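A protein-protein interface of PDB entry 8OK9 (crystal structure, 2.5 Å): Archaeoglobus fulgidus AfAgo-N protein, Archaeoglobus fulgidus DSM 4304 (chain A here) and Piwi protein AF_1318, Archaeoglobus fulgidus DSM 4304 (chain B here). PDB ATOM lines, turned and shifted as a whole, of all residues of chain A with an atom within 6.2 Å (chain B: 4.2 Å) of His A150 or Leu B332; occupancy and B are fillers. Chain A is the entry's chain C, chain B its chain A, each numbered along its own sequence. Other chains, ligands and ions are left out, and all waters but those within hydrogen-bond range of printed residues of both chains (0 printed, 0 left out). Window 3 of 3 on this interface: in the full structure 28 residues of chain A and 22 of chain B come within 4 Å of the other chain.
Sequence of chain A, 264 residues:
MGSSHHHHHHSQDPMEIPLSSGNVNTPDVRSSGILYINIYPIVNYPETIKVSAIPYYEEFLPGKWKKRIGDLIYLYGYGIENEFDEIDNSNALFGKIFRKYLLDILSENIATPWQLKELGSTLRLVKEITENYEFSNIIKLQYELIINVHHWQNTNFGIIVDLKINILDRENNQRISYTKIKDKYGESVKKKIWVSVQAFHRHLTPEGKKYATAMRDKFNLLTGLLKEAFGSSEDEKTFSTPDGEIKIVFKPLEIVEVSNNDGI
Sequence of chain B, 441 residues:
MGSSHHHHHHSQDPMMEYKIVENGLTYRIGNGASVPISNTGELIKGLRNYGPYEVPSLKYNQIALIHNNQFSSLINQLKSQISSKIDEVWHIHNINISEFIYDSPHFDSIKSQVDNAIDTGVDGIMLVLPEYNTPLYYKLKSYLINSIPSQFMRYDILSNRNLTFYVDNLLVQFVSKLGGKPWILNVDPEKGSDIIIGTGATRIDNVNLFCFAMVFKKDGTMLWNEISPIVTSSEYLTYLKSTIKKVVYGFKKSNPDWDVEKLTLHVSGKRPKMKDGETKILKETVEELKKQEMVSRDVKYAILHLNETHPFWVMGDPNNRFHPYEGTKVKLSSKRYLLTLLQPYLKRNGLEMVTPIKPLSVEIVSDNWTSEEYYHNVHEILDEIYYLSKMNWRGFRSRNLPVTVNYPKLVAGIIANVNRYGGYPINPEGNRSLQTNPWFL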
ATOM      1  N   ILE A  37      -5.515  -6.720  19.725  1.00  0.00           N
ATOM      2  CA  ILE A  37      -6.704  -6.794  20.623  1.00  0.00           C
ATOM      3  C   ILE A  37      -6.490  -5.793  21.760  1.00  0.00           C
ATOM      4  O   ILE A  37      -5.330  -5.457  22.025  1.00  0.00           O
ATOM      5  CB  ILE A  37      -6.931  -8.240  21.115  1.00  0.00           C
ATOM      6  CG1 ILE A  37      -8.288  -8.436  21.792  1.00  0.00           C
ATOM      7  CG2 ILE A  37      -5.782  -8.731  21.981  1.00  0.00           C
ATOM      8  CD1 ILE A  37      -8.787  -9.849  21.720  1.00  0.00           C
ATOM      9  N   ILE A  39      -6.047  -5.888  24.751  1.00  0.00           N
ATOM     10  CA  ILE A  39      -5.543  -6.576  25.969  1.00  0.00           C
ATOM     11  C   ILE A  39      -4.092  -6.123  26.104  1.00  0.00           C
ATOM     12  O   ILE A  39      -3.340  -6.262  25.132  1.00  0.00           O
ATOM     13  CB  ILE A  39      -5.656  -8.109  25.850  1.00  0.00           C
ATOM     14  CG1 ILE A  39      -7.105  -8.569  25.682  1.00  0.00           C
ATOM     15  CG2 ILE A  39      -4.988  -8.798  27.030  1.00  0.00           C
ATOM     16  CD1 ILE A  39      -7.251 -10.063  25.537  1.00  0.00           C
ATOM     17  N   ILE A  42       0.768  -7.963  31.093  1.00  0.00           N
ATOM     18  CA  ILE A  42       1.620  -7.703  32.291  1.00  0.00           C
ATOM     19  C   ILE A  42       2.799  -8.661  32.140  1.00  0.00           C
ATOM     20  O   ILE A  42       2.701  -9.802  32.635  1.00  0.00           O
ATOM     21  CB  ILE A  42       0.824  -7.894  33.594  1.00  0.00           C
ATOM     22  CG1 ILE A  42      -0.515  -7.161  33.517  1.00  0.00           C
ATOM     23  CG2 ILE A  42       1.627  -7.437  34.799  1.00  0.00           C
ATOM     24  CD1 ILE A  42      -1.665  -7.973  34.024  1.00  0.00           C
ATOM     25  N   ARG A  99      -6.121 -12.050  39.611  1.00  0.00           N
ATOM     26  CA  ARG A  99      -6.978 -11.278  38.716  1.00  0.00           C
ATOM     27  C   ARG A  99      -7.620 -10.102  39.445  1.00  0.00           C
ATOM     28  O   ARG A  99      -7.804  -9.028  38.860  1.00  0.00           O
ATOM     29  CB  ARG A  99      -8.043 -12.182  38.096  1.00  0.00           C
ATOM     30  CG  ARG A  99      -7.607 -12.828  36.787  1.00  0.00           C
ATOM     31  CD  ARG A  99      -8.666 -13.766  36.231  1.00  0.00           C
ATOM     32  NE  ARG A  99      -9.689 -13.043  35.478  1.00  0.00           N
ATOM     33  CZ  ARG A  99     -10.941 -12.880  35.890  1.00  0.00           C
ATOM     34  NH1 ARG A  99     -11.331 -13.392  37.049  1.00  0.00           N
ATOM     35  NH2 ARG A  99     -11.805 -12.206  35.142  1.00  0.00           N
ATOM     36  N   LEU A 102      -4.658  -7.690  41.065  1.00  0.00           N
ATOM     37  CA  LEU A 102      -4.086  -6.804  40.017  1.00  0.00           C
ATOM     38  C   LEU A 102      -4.867  -5.497  40.032  1.00  0.00           C
ATOM     39  O   LEU A 102      -4.234  -4.427  40.069  1.00  0.00           O
ATOM     40  CB  LEU A 102      -4.364  -7.478  38.674  1.00  0.00           C
ATOM     41  CG  LEU A 102      -3.933  -6.724  37.425  1.00  0.00           C
ATOM     42  CD1 LEU A 102      -2.425  -6.539  37.394  1.00  0.00           C
ATOM     43  CD2 LEU A 102      -4.417  -7.468  36.194  1.00  0.00           C
ATOM     44  N   ASN A 148     -10.673  -4.818  32.932  1.00  0.00           N
ATOM     45  CA  ASN A 148     -10.762  -6.186  33.425  1.00  0.00           C
ATOM     46  C   ASN A 148      -9.397  -6.850  33.277  1.00  0.00           C
ATOM     47  O   ASN A 148      -8.458  -6.266  32.733  1.00  0.00           O
ATOM     48  CB  ASN A 148     -11.840  -6.971  32.674  1.00  0.00           C
ATOM     49  CG  ASN A 148     -13.242  -6.550  33.060  1.00  0.00           C
ATOM     50  OD1 ASN A 148     -13.768  -6.973  34.089  1.00  0.00           O
ATOM     51  ND2 ASN A 148     -13.857  -5.713  32.232  1.00  0.00           N
ATOM     52  N   VAL A 149      -9.285  -8.083  33.763  1.00  0.00           N
ATOM     53  CA  VAL A 149      -8.051  -8.854  33.676  1.00  0.00           C
ATOM     54  C   VAL A 149      -8.320 -10.112  32.864  1.00  0.00           C
ATOM     55  O   VAL A 149      -9.280 -10.841  33.139  1.00  0.00           O
ATOM     56  CB  VAL A 149      -7.498  -9.214  35.066  1.00  0.00           C
ATOM     57  CG1 VAL A 149      -6.255 -10.080  34.927  1.00  0.00           C
ATOM     58  CG2 VAL A 149      -7.182  -7.955  35.855  1.00  0.00           C
ATOM     59  N   HIS A 150      -7.476 -10.362  31.867  1.00  0.00           N
ATOM     60  CA  HIS A 150      -7.546 -11.577  31.069  1.00  0.00           C
ATOM     61  C   HIS A 150      -6.449 -12.542  31.496  1.00  0.00           C
ATOM     62  O   HIS A 150      -5.314 -12.134  31.758  1.00  0.00           O
ATOM     63  CB  HIS A 150      -7.412 -11.267  29.578  1.00  0.00           C
ATOM     64  CG  HIS A 150      -7.811 -12.407  28.694  1.00  0.00           C
ATOM     65  ND1 HIS A 150      -9.086 -12.930  28.687  1.00  0.00           N
ATOM     66  CD2 HIS A 150      -7.102 -13.131  27.798  1.00  0.00           C
ATOM     67  CE1 HIS A 150      -9.146 -13.924  27.819  1.00  0.00           C
ATOM     68  NE2 HIS A 150      -7.955 -14.066  27.266  1.00  0.00           N
ATOM     69  N   HIS A 151      -6.794 -13.827  31.556  1.00  0.00           N
ATOM     70  CA  HIS A 151      -5.893 -14.862  32.049  1.00  0.00           C
ATOM     71  C   HIS A 151      -5.905 -16.014  31.059  1.00  0.00           C
ATOM     72  O   HIS A 151      -6.915 -16.712  30.913  1.00  0.00           O
ATOM     73  CB  HIS A 151      -6.301 -15.321  33.448  1.00  0.00           C
ATOM     74  CG  HIS A 151      -5.468 -16.438  33.999  1.00  0.00           C
ATOM     75  ND1 HIS A 151      -5.915 -17.262  35.010  1.00  0.00           N
ATOM     76  CD2 HIS A 151      -4.222 -16.867  33.689  1.00  0.00           C
ATOM     77  CE1 HIS A 151      -4.981 -18.149  35.299  1.00  0.00           C
ATOM     78  NE2 HIS A 151      -3.943 -17.932  34.510  1.00  0.00           N
ATOM     79  N   TRP A 152      -4.841 -16.068  30.255  1.00  0.00           N
ATOM     80  CA  TRP A 152      -4.750 -17.102  29.197  1.00  0.00           C
ATOM     81  C   TRP A 152      -3.466 -17.902  29.401  1.00  0.00           C
ATOM     82  O   TRP A 152      -2.737 -17.570  30.354  1.00  0.00           O
ATOM     83  CB  TRP A 152      -4.891 -16.489  27.796  1.00  0.00           C
ATOM     84  CG  TRP A 152      -3.716 -15.728  27.263  1.00  0.00           C
ATOM     85  CD1 TRP A 152      -2.842 -16.151  26.304  1.00  0.00           C
ATOM     86  CD2 TRP A 152      -3.321 -14.384  27.595  1.00  0.00           C
ATOM     87  NE1 TRP A 152      -1.915 -15.180  26.042  1.00  0.00           N
ATOM     88  CE2 TRP A 152      -2.185 -14.083  26.814  1.00  0.00           C
ATOM     89  CE3 TRP A 152      -3.800 -13.414  28.482  1.00  0.00           C
ATOM     90  CZ2 TRP A 152      -1.523 -12.861  26.902  1.00  0.00           C
ATOM     91  CZ3 TRP A 152      -3.153 -12.203  28.559  1.00  0.00           C
ATOM     92  CH2 TRP A 152      -2.027 -11.932  27.783  1.00  0.00           C
ATOM     93  N   GLN A 153      -3.224 -18.917  28.571  1.00  0.00           N
ATOM     94  CA  GLN A 153      -2.081 -19.841  28.785  1.00  0.00           C
ATOM     95  C   GLN A 153      -2.257 -20.348  30.212  1.00  0.00           C
ATOM     96  O   GLN A 153      -3.375 -20.782  30.538  1.00  0.00           O
ATOM     97  CB  GLN A 153      -0.736 -19.183  28.472  1.00  0.00           C
ATOM     98  CG  GLN A 153      -0.570 -18.837  27.000  1.00  0.00           C
ATOM     99  CD  GLN A 153      -0.655 -20.044  26.098  1.00  0.00           C
ATOM    100  OE1 GLN A 153      -0.138 -21.114  26.412  1.00  0.00           O
ATOM    101  NE2 GLN A 153      -1.320 -19.882  24.967  1.00  0.00           N
ATOM    102  N   ASN A 156      -0.122 -16.349  31.749  1.00  0.00           N
ATOM    103  CA  ASN A 156      -0.221 -15.085  30.972  1.00  0.00           C
ATOM    104  C   ASN A 156      -1.368 -14.209  31.487  1.00  0.00           C
ATOM    105  O   ASN A 156      -2.493 -14.721  31.586  1.00  0.00           O
ATOM    106  CB  ASN A 156      -0.269 -15.361  29.469  1.00  0.00           C
ATOM    107  CG  ASN A 156       1.104 -15.428  28.836  1.00  0.00           C
ATOM    108  OD1 ASN A 156       2.114 -15.443  29.535  1.00  0.00           O
ATOM    109  ND2 ASN A 156       1.151 -15.465  27.516  1.00  0.00           N
ATOM    110  N   PHE A 157      -1.081 -12.942  31.816  1.00  0.00           N
ATOM    111  CA  PHE A 157      -2.095 -12.021  32.306  1.00  0.00           C
ATOM    112  C   PHE A 157      -2.018 -10.716  31.528  1.00  0.00           C
ATOM    113  O   PHE A 157      -0.957 -10.329  31.032  1.00  0.00           O
ATOM    114  CB  PHE A 157      -1.934 -11.730  33.808  1.00  0.00           C
ATOM    115  CG  PHE A 157      -2.107 -12.937  34.687  1.00  0.00           C
ATOM    116  CD1 PHE A 157      -1.045 -13.790  34.934  1.00  0.00           C
ATOM    117  CD2 PHE A 157      -3.333 -13.213  35.272  1.00  0.00           C
ATOM    118  CE1 PHE A 157      -1.201 -14.899  35.745  1.00  0.00           C
ATOM    119  CE2 PHE A 157      -3.495 -14.321  36.084  1.00  0.00           C
ATOM    120  CZ  PHE A 157      -2.427 -15.165  36.321  1.00  0.00           C
ATOM    121  N   GLY A 158      -3.160 -10.047  31.428  1.00  0.00           N
ATOM    122  CA  GLY A 158      -3.227  -8.747  30.789  1.00  0.00           C
ATOM    123  C   GLY A 158      -4.509  -8.056  31.185  1.00  0.00           C
ATOM    124  O   GLY A 158      -5.449  -8.686  31.678  1.00  0.00           O
ATOM    125  N   ILE A 159      -4.539  -6.743  30.971  1.00  0.00           N
ATOM    126  CA  ILE A 159      -5.708  -5.937  31.297  1.00  0.00           C
ATOM    127  C   ILE A 159      -6.487  -5.656  30.020  1.00  0.00           C
ATOM    128  O   ILE A 159      -5.929  -5.165  29.029  1.00  0.00           O
ATOM    129  CB  ILE A 159      -5.323  -4.632  32.020  1.00  0.00           C
ATOM    130  CG1 ILE A 159      -4.246  -3.863  31.254  1.00  0.00           C
ATOM    131  CG2 ILE A 159      -4.865  -4.929  33.443  1.00  0.00           C
ATOM    132  CD1 ILE A 159      -3.933  -2.511  31.858  1.00  0.00           C
ATOM    133  N   ILE A 160      -7.768  -5.994  30.039  1.00  0.00           N
ATOM    134  CA  ILE A 160      -8.690  -5.664  28.960  1.00  0.00           C
ATOM    135  C   ILE A 160      -9.231  -4.274  29.264  1.00  0.00           C
ATOM    136  O   ILE A 160      -9.824  -4.060  30.327  1.00  0.00           O
ATOM    137  CB  ILE A 160      -9.830  -6.690  28.886  1.00  0.00           C
ATOM    138  CG1 ILE A 160      -9.269  -8.111  28.858  1.00  0.00           C
ATOM    139  CG2 ILE A 160     -10.701  -6.436  27.663  1.00  0.00           C
ATOM    140  CD1 ILE A 160     -10.300  -9.168  29.186  1.00  0.00           C
ATOM    141  N   MET B  16      -4.815 -17.422  21.763  1.00  0.00           N
ATOM    142  CA  MET B  16      -4.452 -16.064  21.336  1.00  0.00           C
ATOM    143  C   MET B  16      -3.714 -16.068  20.002  1.00  0.00           C
ATOM    144  O   MET B  16      -2.892 -15.192  19.716  1.00  0.00           O
ATOM    145  CB  MET B  16      -3.651 -15.327  22.408  1.00  0.00           C
ATOM    146  CG  MET B  16      -4.038 -13.858  22.525  1.00  0.00           C
ATOM    147  SD  MET B  16      -5.761 -13.588  22.991  1.00  0.00           S
ATOM    148  CE  MET B  16      -5.662 -13.749  24.770  1.00  0.00           C
ATOM    149  N   PHE B 312     -14.253  -6.591  24.131  1.00  0.00           N
ATOM    150  CA  PHE B 312     -13.139  -6.833  23.225  1.00  0.00           C
ATOM    151  C   PHE B 312     -13.309  -6.110  21.893  1.00  0.00           C
ATOM    152  O   PHE B 312     -14.420  -5.954  21.378  1.00  0.00           O
ATOM    153  CB  PHE B 312     -12.973  -8.332  22.977  1.00  0.00           C
ATOM    154  CG  PHE B 312     -12.607  -9.108  24.206  1.00  0.00           C
ATOM    155  CD1 PHE B 312     -11.316  -9.066  24.706  1.00  0.00           C
ATOM    156  CD2 PHE B 312     -13.555  -9.866  24.871  1.00  0.00           C
ATOM    157  CE1 PHE B 312     -10.977  -9.776  25.839  1.00  0.00           C
ATOM    158  CE2 PHE B 312     -13.224 -10.575  26.007  1.00  0.00           C
ATOM    159  CZ  PHE B 312     -11.932 -10.533  26.489  1.00  0.00           C
ATOM    160  N   VAL B 330     -10.563 -15.667  16.552  1.00  0.00           N
ATOM    161  CA  VAL B 330      -9.545 -15.431  17.567  1.00  0.00           C
ATOM    162  C   VAL B 330      -9.844 -16.320  18.764  1.00  0.00           C
ATOM    163  O   VAL B 330     -10.981 -16.362  19.247  1.00  0.00           O
ATOM    164  CB  VAL B 330      -9.511 -13.950  17.978  1.00  0.00           C
ATOM    165  CG1 VAL B 330      -8.642 -13.757  19.214  1.00  0.00           C
ATOM    166  CG2 VAL B 330      -9.011 -13.091  16.830  1.00  0.00           C
ATOM    167  N   LYS B 331      -8.831 -17.037  19.243  1.00  0.00           N
ATOM    168  CA  LYS B 331      -8.977 -17.875  20.427  1.00  0.00           C
ATOM    169  C   LYS B 331      -8.565 -17.063  21.650  1.00  0.00           C
ATOM    170  O   LYS B 331      -7.376 -16.809  21.863  1.00  0.00           O
ATOM    171  CB  LYS B 331      -8.145 -19.148  20.305  1.00  0.00           C
ATOM    172  CG  LYS B 331      -8.436 -20.156  21.403  1.00  0.00           C
ATOM    173  CD  LYS B 331      -7.705 -21.469  21.193  1.00  0.00           C
ATOM    174  CE  LYS B 331      -8.201 -22.527  22.168  1.00  0.00           C
ATOM    175  NZ  LYS B 331      -7.527 -23.840  21.973  1.00  0.00           N
ATOM    176  N   LEU B 332      -9.549 -16.649  22.451  1.00  0.00           N
ATOM    177  CA  LEU B 332      -9.247 -15.870  23.647  1.00  0.00           C
ATOM    178  C   LEU B 332      -8.632 -16.740  24.732  1.00  0.00           C
ATOM    179  O   LEU B 332      -7.681 -16.329  25.406  1.00  0.00           O
ATOM    180  CB  LEU B 332     -10.515 -15.201  24.168  1.00  0.00           C
ATOM    181  CG  LEU B 332     -10.903 -13.867  23.539  1.00  0.00           C
ATOM    182  CD1 LEU B 332     -12.132 -13.322  24.238  1.00  0.00           C
ATOM    183  CD2 LEU B 332      -9.748 -12.882  23.617  1.00  0.00           C
ATOM    184  N   SER B 333      -9.169 -17.940  24.918  1.00  0.00           N
ATOM    185  CA  SER B 333      -8.714 -18.864  25.945  1.00  0.00           C
ATOM    186  C   SER B 333      -9.093 -20.272  25.499  1.00  0.00           C
ATOM    187  O   SER B 333      -9.445 -20.495  24.336  1.00  0.00           O
ATOM    188  CB  SER B 333      -9.305 -18.493  27.309  1.00  0.00           C
ATOM    189  OG  SER B 333     -10.720 -18.439  27.252  1.00  0.00           O
ATOM    190  N   ARG B 336     -13.053 -20.182  24.709  1.00  0.00           N
ATOM    191  CA  ARG B 336     -13.722 -18.948  24.325  1.00  0.00           C
ATOM    192  C   ARG B 336     -13.067 -18.365  23.081  1.00  0.00           C
ATOM    193  O   ARG B 336     -11.837 -18.325  22.974  1.00  0.00           O
ATOM    194  CB  ARG B 336     -13.693 -17.918  25.458  1.00  0.00           C
ATOM    195  CG  ARG B 336     -14.468 -16.654  25.139  1.00  0.00           C
ATOM    196  CD  ARG B 336     -14.403 -15.650  26.271  1.00  0.00           C
ATOM    197  NE  ARG B 336     -15.308 -14.529  26.040  1.00  0.00           N
ATOM    198  CZ  ARG B 336     -15.442 -13.496  26.864  1.00  0.00           C
ATOM    199  NH1 ARG B 336     -14.728 -13.439  27.979  1.00  0.00           N
ATOM    200  NH2 ARG B 336     -16.292 -12.521  26.572  1.00  0.00           N
ATOM    201  N   LEU B 338     -13.445 -15.276  19.711  1.00  0.00           N
ATOM    202  CA  LEU B 338     -14.020 -14.078  19.113  1.00  0.00           C
ATOM    203  C   LEU B 338     -14.132 -14.291  17.612  1.00  0.00           C
ATOM    204  O   LEU B 338     -13.140 -14.625  16.954  1.00  0.00           O
ATOM    205  CB  LEU B 338     -13.174 -12.840  19.410  1.00  0.00           C
ATOM    206  CG  LEU B 338     -13.069 -12.421  20.875  1.00  0.00           C
ATOM    207  CD1 LEU B 338     -12.055 -11.301  21.034  1.00  0.00           C
ATOM    208  CD2 LEU B 338     -14.430 -12.005  21.415  1.00  0.00           C
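O of Leu B332 lies within hydrogen-bond range of NE2 of His A150, 2.9 Å away.
The side-chain amide nitrogen (ND2) of Asn A156 sits close to the indole nitrogen (NE1) of Trp A152 (3.4 Å). The backbone carbonyl oxygen of Val B330 lies within hydrogen-bond range of the backbone NH of Leu B338 (2.7 Å). The backbone carbonyl oxygen (O) of Asn A148 sits at hydrogen-bond distance from the backbone NH (N) of Ile A160 (2.8 Å). O of Gly A158 is in hydrogen-bond range of N of His A150, at 2.6 Å. The backbone NH (N) of Met B16 lies within hydrogen-bond range of the backbone carbonyl oxygen (O) of Lys B331.
Ile A37 touches Phe B312 (CD1 to CD1, 3.99 Å). Leu B332 touches Ile A37 (CD2 to CD1, 3.7 Å). Leu B338 touches Ile A37. Ile A39 touches Phe B312 (CD1 to CE1, 3.7 Å). Met B16 touches His A150 (CE to NE2, 3.4 Å). Trp A152 touches Met B16. CB of Trp A152 touches O of Leu B332, 3.7 Å away. Ile A160 touches Phe B312.
His A150 touches just these residues of chain B: Met B16 and Leu B332. Leu B332 touches just these residues of chain A: Ile A37 (3.7 Å), His A150 (2.9 Å) and Trp A152 (3.7 Å). Printed residues of chain B within 4 Å of Ile A37: Phe B312, Leu B332 and Leu B338. Of the printed residues of chain B, Ile A160 touches Phe B312 (3.4 Å). Ser B333 touches none of the printed residues of chain A. The nearest printed residue of chain B that does not touch His A150 is Phe B312 (4.3 Å). The nearest residue of chain A that does not touch Leu B332 is Ile A39 (4.2 Å).
Of the 16 printed residues of chain A, 5 touch a printed residue of chain B. Hydrophobic or aromatic side chains of chain A within 4 Å of the printed part of chain B: Ile A37, Ile A39, His A150, Trp A152 and Ile A160. Of the 8 printed residues of chain B, 4 touch a printed residue of chain A. Among the printed residues, 9 pairs touch across the chains. Among the printed residues, no Asp or Glu carboxylate lies within 4 Å of a Lys or Arg side-chain nitrogen of the other chain.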
